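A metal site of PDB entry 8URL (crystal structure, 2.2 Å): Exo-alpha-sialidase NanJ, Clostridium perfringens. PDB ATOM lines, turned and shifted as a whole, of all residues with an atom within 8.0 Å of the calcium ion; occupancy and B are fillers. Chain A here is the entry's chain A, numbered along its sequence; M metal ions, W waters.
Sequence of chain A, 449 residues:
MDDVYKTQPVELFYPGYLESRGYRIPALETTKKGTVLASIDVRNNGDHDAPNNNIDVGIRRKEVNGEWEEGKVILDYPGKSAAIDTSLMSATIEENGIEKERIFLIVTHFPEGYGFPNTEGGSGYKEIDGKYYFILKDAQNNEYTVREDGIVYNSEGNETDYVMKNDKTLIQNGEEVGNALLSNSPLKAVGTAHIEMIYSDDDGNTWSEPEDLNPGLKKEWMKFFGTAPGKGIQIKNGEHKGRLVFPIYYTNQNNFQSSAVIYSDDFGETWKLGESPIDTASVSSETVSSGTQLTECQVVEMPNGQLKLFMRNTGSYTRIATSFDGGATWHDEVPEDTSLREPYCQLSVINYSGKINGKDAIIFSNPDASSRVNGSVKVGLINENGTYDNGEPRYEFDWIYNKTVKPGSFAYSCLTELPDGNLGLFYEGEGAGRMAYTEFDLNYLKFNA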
ATOM      1  N   THR A 292       6.954  29.635  20.969  1.00  0.00           N
ATOM      2  CA  THR A 292       7.763  28.453  20.748  1.00  0.00           C
ATOM      3  C   THR A 292       7.810  28.112  19.256  1.00  0.00           C
ATOM      4  O   THR A 292       6.761  27.938  18.619  1.00  0.00           O
ATOM      5  CB  THR A 292       7.213  27.290  21.542  1.00  0.00           C
ATOM      6  OG1 THR A 292       7.293  27.596  22.937  1.00  0.00           O
ATOM      7  CG2 THR A 292       8.031  26.004  21.259  1.00  0.00           C
ATOM      8  N   GLN A 293       9.011  28.020  18.701  1.00  0.00           N
ATOM      9  CA  GLN A 293       9.157  27.631  17.302  1.00  0.00           C
ATOM     10  C   GLN A 293       9.173  26.115  17.204  1.00  0.00           C
ATOM     11  O   GLN A 293       9.690  25.436  18.093  1.00  0.00           O
ATOM     12  CB  GLN A 293      10.420  28.216  16.701  1.00  0.00           C
ATOM     13  CG  GLN A 293      10.388  29.732  16.553  1.00  0.00           C
ATOM     14  CD  GLN A 293      11.666  30.241  15.934  1.00  0.00           C
ATOM     15  OE1 GLN A 293      11.819  30.277  14.717  1.00  0.00           O
ATOM     16  NE2 GLN A 293      12.615  30.610  16.791  1.00  0.00           N
ATOM     17  N   THR A 295      10.338  23.107  14.683  1.00  0.00           N
ATOM     18  CA  THR A 295      11.302  23.099  13.594  1.00  0.00           C
ATOM     19  C   THR A 295      11.373  21.685  13.005  1.00  0.00           C
ATOM     20  O   THR A 295      10.368  21.209  12.483  1.00  0.00           O
ATOM     21  CB  THR A 295      12.652  23.689  14.047  1.00  0.00           C
ATOM     22  OG1 THR A 295      13.409  22.725  14.781  1.00  0.00           O
ATOM     23  CG2 THR A 295      12.427  24.904  14.942  1.00  0.00           C
ATOM     24  N   MET A 311       8.232  17.009  17.282  1.00  0.00           N
ATOM     25  CA  MET A 311       8.874  18.231  16.798  1.00  0.00           C
ATOM     26  C   MET A 311       9.977  18.705  17.721  1.00  0.00           C
ATOM     27  O   MET A 311       9.749  18.940  18.913  1.00  0.00           O
ATOM     28  CB  MET A 311       7.832  19.357  16.644  1.00  0.00           C
ATOM     29  CG  MET A 311       6.879  19.157  15.486  1.00  0.00           C
ATOM     30  SD  MET A 311       5.451  20.228  15.548  1.00  0.00           S
ATOM     31  CE  MET A 311       4.659  19.696  17.052  1.00  0.00           C
ATOM     32  N   ARG A 312      11.172  18.876  17.155  1.00  0.00           N
ATOM     33  CA  ARG A 312      12.171  19.749  17.755  1.00  0.00           C
ATOM     34  C   ARG A 312      11.541  21.130  17.918  1.00  0.00           C
ATOM     35  O   ARG A 312      10.746  21.566  17.094  1.00  0.00           O
ATOM     36  CB  ARG A 312      13.407  19.819  16.848  1.00  0.00           C
ATOM     37  CG  ARG A 312      14.475  20.858  17.243  1.00  0.00           C
ATOM     38  CD  ARG A 312      15.620  20.884  16.198  1.00  0.00           C
ATOM     39  NE  ARG A 312      16.614  21.907  16.487  1.00  0.00           N
ATOM     40  CZ  ARG A 312      17.844  21.948  15.977  1.00  0.00           C
ATOM     41  NH1 ARG A 312      18.274  21.041  15.124  1.00  0.00           N
ATOM     42  NH2 ARG A 312      18.669  22.944  16.327  1.00  0.00           N
ATOM     43  N   ASN A 313      11.866  21.802  19.013  1.00  0.00           N
ATOM     44  CA  ASN A 313      11.267  23.101  19.285  1.00  0.00           C
ATOM     45  C   ASN A 313      12.144  23.833  20.274  1.00  0.00           C
ATOM     46  O   ASN A 313      13.070  23.268  20.859  1.00  0.00           O
ATOM     47  CB  ASN A 313       9.825  22.937  19.808  1.00  0.00           C
ATOM     48  CG  ASN A 313       9.787  22.299  21.160  1.00  0.00           C
ATOM     49  OD1 ASN A 313       9.790  22.977  22.180  1.00  0.00           O
ATOM     50  ND2 ASN A 313       9.783  20.969  21.187  1.00  0.00           N
ATOM     51  N   THR A 314      11.847  25.123  20.462  1.00  0.00           N
ATOM     52  CA  THR A 314      12.678  25.929  21.359  1.00  0.00           C
ATOM     53  C   THR A 314      12.314  25.750  22.835  1.00  0.00           C
ATOM     54  O   THR A 314      12.912  26.425  23.688  1.00  0.00           O
ATOM     55  CB  THR A 314      12.593  27.402  20.979  1.00  0.00           C
ATOM     56  OG1 THR A 314      11.240  27.725  20.700  1.00  0.00           O
ATOM     57  CG2 THR A 314      13.446  27.705  19.762  1.00  0.00           C
ATOM     58  N   GLY A 315      11.357  24.896  23.166  1.00  0.00           N
ATOM     59  CA  GLY A 315      11.055  24.559  24.538  1.00  0.00           C
ATOM     60  C   GLY A 315      11.938  23.434  25.041  1.00  0.00           C
ATOM     61  O   GLY A 315      12.857  22.961  24.379  1.00  0.00           O
ATOM     62  N   SER A 316      11.653  23.009  26.269  1.00  0.00           N
ATOM     63  CA  SER A 316      12.496  22.026  26.914  1.00  0.00           C
ATOM     64  C   SER A 316      12.134  20.591  26.537  1.00  0.00           C
ATOM     65  O   SER A 316      12.985  19.703  26.666  1.00  0.00           O
ATOM     66  CB  SER A 316      12.425  22.204  28.430  1.00  0.00           C
ATOM     67  OG  SER A 316      12.810  23.519  28.819  1.00  0.00           O
ATOM     68  N   TYR A 317      10.927  20.357  26.047  1.00  0.00           N
ATOM     69  CA  TYR A 317      10.457  19.008  25.759  1.00  0.00           C
ATOM     70  C   TYR A 317       9.903  18.925  24.356  1.00  0.00           C
ATOM     71  O   TYR A 317       9.495  19.927  23.755  1.00  0.00           O
ATOM     72  CB  TYR A 317       9.381  18.577  26.773  1.00  0.00           C
ATOM     73  CG  TYR A 317       9.921  18.552  28.176  1.00  0.00           C
ATOM     74  CD1 TYR A 317      10.656  17.466  28.625  1.00  0.00           C
ATOM     75  CD2 TYR A 317       9.727  19.621  29.028  1.00  0.00           C
ATOM     76  CE1 TYR A 317      11.169  17.434  29.896  1.00  0.00           C
ATOM     77  CE2 TYR A 317      10.239  19.600  30.316  1.00  0.00           C
ATOM     78  CZ  TYR A 317      10.966  18.498  30.738  1.00  0.00           C
ATOM     79  OH  TYR A 317      11.492  18.468  31.998  1.00  0.00           O
ATOM     80  N   THR A 318       9.891  17.704  23.843  1.00  0.00           N
ATOM     81  CA  THR A 318       9.309  17.392  22.546  1.00  0.00           C
ATOM     82  C   THR A 318       7.828  17.781  22.501  1.00  0.00           C
ATOM     83  O   THR A 318       7.050  17.389  23.373  1.00  0.00           O
ATOM     84  CB  THR A 318       9.472  15.890  22.283  1.00  0.00           C
ATOM     85  OG1 THR A 318      10.862  15.535  22.345  1.00  0.00           O
ATOM     86  CG2 THR A 318       8.881  15.490  20.924  1.00  0.00           C
ATOM     87  N   ARG A 319       7.449  18.527  21.470  1.00  0.00           N
ATOM     88  CA  ARG A 319       6.054  18.833  21.186  1.00  0.00           C
ATOM     89  C   ARG A 319       5.490  17.819  20.205  1.00  0.00           C
ATOM     90  O   ARG A 319       6.144  17.461  19.228  1.00  0.00           O
ATOM     91  CB  ARG A 319       5.911  20.233  20.582  1.00  0.00           C
ATOM     92  CG  ARG A 319       6.266  21.365  21.496  1.00  0.00           C
ATOM     93  CD  ARG A 319       5.101  21.655  22.418  1.00  0.00           C
ATOM     94  NE  ARG A 319       5.379  22.800  23.267  1.00  0.00           N
ATOM     95  CZ  ARG A 319       4.491  23.383  24.052  1.00  0.00           C
ATOM     96  NH1 ARG A 319       3.246  22.954  24.120  1.00  0.00           N
ATOM     97  NH2 ARG A 319       4.860  24.428  24.784  1.00  0.00           N
ATOM     98  N   GLU A 336       3.419  19.338  25.184  1.00  0.00           N
ATOM     99  CA  GLU A 336       4.711  18.709  25.424  1.00  0.00           C
ATOM    100  C   GLU A 336       4.513  17.287  25.922  1.00  0.00           C
ATOM    101  O   GLU A 336       3.494  16.960  26.541  1.00  0.00           O
ATOM    102  CB  GLU A 336       5.517  19.512  26.454  1.00  0.00           C
ATOM    103  CG  GLU A 336       6.248  20.719  25.869  1.00  0.00           C
ATOM    104  CD  GLU A 336       7.135  21.402  26.880  1.00  0.00           C
ATOM    105  OE1 GLU A 336       6.774  21.408  28.082  1.00  0.00           O
ATOM    106  OE2 GLU A 336       8.206  21.918  26.490  1.00  0.00           O
ATOM    107  N   LEU A 340      10.252  13.360  27.222  1.00  0.00           N
ATOM    108  CA  LEU A 340      11.081  13.476  26.009  1.00  0.00           C
ATOM    109  C   LEU A 340      11.805  14.807  26.032  1.00  0.00           C
ATOM    110  O   LEU A 340      11.466  15.706  25.266  1.00  0.00           O
ATOM    111  CB  LEU A 340      10.227  13.326  24.743  1.00  0.00           C
ATOM    112  CG  LEU A 340       9.379  12.061  24.661  1.00  0.00           C
ATOM    113  CD1 LEU A 340       8.620  11.935  23.339  1.00  0.00           C
ATOM    114  CD2 LEU A 340      10.315  10.892  24.859  1.00  0.00           C
ATOM    115  N   ARG A 341      12.778  14.922  26.921  1.00  0.00           N
ATOM    116  CA  ARG A 341      13.614  16.116  26.965  1.00  0.00           C
ATOM    117  C   ARG A 341      14.237  16.330  25.602  1.00  0.00           C
ATOM    118  O   ARG A 341      14.638  15.375  24.924  1.00  0.00           O
ATOM    119  CB  ARG A 341      14.683  15.961  28.038  1.00  0.00           C
ATOM    120  CG  ARG A 341      15.527  17.201  28.283  1.00  0.00           C
ATOM    121  CD  ARG A 341      14.709  18.349  28.855  1.00  0.00           C
ATOM    122  NE  ARG A 341      15.593  19.396  29.360  1.00  0.00           N
ATOM    123  CZ  ARG A 341      16.118  20.360  28.627  1.00  0.00           C
ATOM    124  NH1 ARG A 341      15.757  20.552  27.359  1.00  0.00           N
ATOM    125  NH2 ARG A 341      17.045  21.150  29.167  1.00  0.00           N
ATOM    126  N   GLU A 342      14.308  17.594  25.187  1.00  0.00           N
ATOM    127  CA  GLU A 342      14.546  17.956  23.791  1.00  0.00           C
ATOM    128  C   GLU A 342      15.469  19.165  23.761  1.00  0.00           C
ATOM    129  O   GLU A 342      15.008  20.317  23.808  1.00  0.00           O
ATOM    130  CB  GLU A 342      13.222  18.250  23.072  1.00  0.00           C
ATOM    131  CG  GLU A 342      13.265  18.194  21.565  1.00  0.00           C
ATOM    132  CD  GLU A 342      14.154  19.264  20.981  1.00  0.00           C
ATOM    133  OE1 GLU A 342      13.667  20.398  20.769  1.00  0.00           O
ATOM    134  OE2 GLU A 342      15.354  18.970  20.785  1.00  0.00           O
ATOM    135  N   PRO A 343      16.809  18.943  23.689  1.00  0.00           N
ATOM    136  CA  PRO A 343      17.761  20.058  23.824  1.00  0.00           C
ATOM    137  C   PRO A 343      18.008  20.798  22.521  1.00  0.00           C
ATOM    138  O   PRO A 343      19.119  21.275  22.272  1.00  0.00           O
ATOM    139  CB  PRO A 343      19.029  19.367  24.312  1.00  0.00           C
ATOM    140  CG  PRO A 343      18.984  18.051  23.643  1.00  0.00           C
ATOM    141  CD  PRO A 343      17.519  17.646  23.646  1.00  0.00           C
ATOM    142  N   TYR A 344      16.981  20.897  21.675  1.00  0.00           N
ATOM    143  CA  TYR A 344      17.044  21.604  20.400  1.00  0.00           C
ATOM    144  C   TYR A 344      17.919  20.819  19.436  1.00  0.00           C
ATOM    145  O   TYR A 344      18.975  21.289  18.990  1.00  0.00           O
ATOM    146  CB  TYR A 344      17.516  23.054  20.582  1.00  0.00           C
ATOM    147  CG  TYR A 344      17.058  23.953  19.475  1.00  0.00           C
ATOM    148  CD1 TYR A 344      15.716  24.026  19.137  1.00  0.00           C
ATOM    149  CD2 TYR A 344      17.956  24.743  18.767  1.00  0.00           C
ATOM    150  CE1 TYR A 344      15.272  24.847  18.121  1.00  0.00           C
ATOM    151  CE2 TYR A 344      17.525  25.579  17.742  1.00  0.00           C
ATOM    152  CZ  TYR A 344      16.187  25.627  17.423  1.00  0.00           C
ATOM    153  OH  TYR A 344      15.741  26.440  16.412  1.00  0.00           O
ATOM    154  N   CYS A 345      17.481  19.602  19.120  1.00  0.00           N
ATOM    155  CA  CYS A 345      18.214  18.717  18.247  1.00  0.00           C
ATOM    156  C   CYS A 345      17.201  17.908  17.443  1.00  0.00           C
ATOM    157  O   CYS A 345      16.074  17.689  17.891  1.00  0.00           O
ATOM    158  CB  CYS A 345      19.152  17.805  19.036  1.00  0.00           C
ATOM    159  SG  CYS A 345      20.118  16.733  17.950  1.00  0.00           S
ATOM    160  N   ASN A 366      16.724  10.287  20.411  1.00  0.00           N
ATOM    161  CA  ASN A 366      17.206  11.672  20.444  1.00  0.00           C
ATOM    162  C   ASN A 366      18.211  11.763  21.585  1.00  0.00           C
ATOM    163  O   ASN A 366      18.392  10.777  22.309  1.00  0.00           O
ATOM    164  CB  ASN A 366      16.045  12.663  20.614  1.00  0.00           C
ATOM    165  CG  ASN A 366      15.798  13.065  22.067  1.00  0.00           C
ATOM    166  OD1 ASN A 366      15.770  12.241  22.975  1.00  0.00           O
ATOM    167  ND2 ASN A 366      15.580  14.360  22.273  1.00  0.00           N
ATOM    168  N   ALA A 369      18.914  14.714  27.195  1.00  0.00           N
ATOM    169  CA  ALA A 369      19.717  15.537  28.089  1.00  0.00           C
ATOM    170  C   ALA A 369      19.426  16.996  27.759  1.00  0.00           C
ATOM    171  O   ALA A 369      18.567  17.303  26.920  1.00  0.00           O
ATOM    172  CB  ALA A 369      21.197  15.225  27.972  1.00  0.00           C
HETATM  173 CA    CA M   1      14.210  21.996  22.455  1.00  0.00          CA
HETATM  174  O   HOH W   1      15.616  23.741  23.580  1.00  0.00           O
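OE2 of Glu 342 lies within hydrogen-bond range of N of Tyr 344 (2.7 Å). The side-chain amide nitrogen of Asn 313 is in hydrogen-bond range of the backbone carbonyl oxygen of Tyr 317 (2.8 Å). O of Ser 316 lies within hydrogen-bond range of N of Glu 342. The backbone NH (N) of Cys 345 lies within hydrogen-bond range of the side-chain carboxylate (OE2) of Glu 342 (2.8 Å). ND2 of Asn 313 lies close to N of Arg 319 (3.4 Å). OD1 of Asn 313 lies within hydrogen-bond range of N of Gly 315, 2.7 Å away. The backbone carbonyl oxygen of Tyr 344 sits close to the guanidinium group of Arg 312 (3.2 Å). The side-chain amide nitrogen of Asn 313 is in hydrogen-bond range of the backbone carbonyl oxygen of Met 311, at 3.0 Å.
Residues that only touch the calcium ion: Pro 343 (3.98 Å). Within 4 Å of the calcium ion: Asn 313, Gly 315, Glu 342, Pro 343 and Tyr 344. The nearest printed residue that does not touch the calcium ion is Thr 314 (4.2 Å).
The calcium ion is bound by the backbone carbonyl oxygen of Glu 342 (2.3 Å), the backbone carbonyl oxygen of Asn 313 (2.3 Å), the side-chain carboxylate of Glu 342 (2.4 Å), water W1 (2.5 Å) and the backbone carbonyl oxygen of Gly 315 (2.5 Å). The calcium ion has five donor atoms within binding distance. Slightly farther from the calcium ion lies N of Tyr 344 (3.1 Å).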
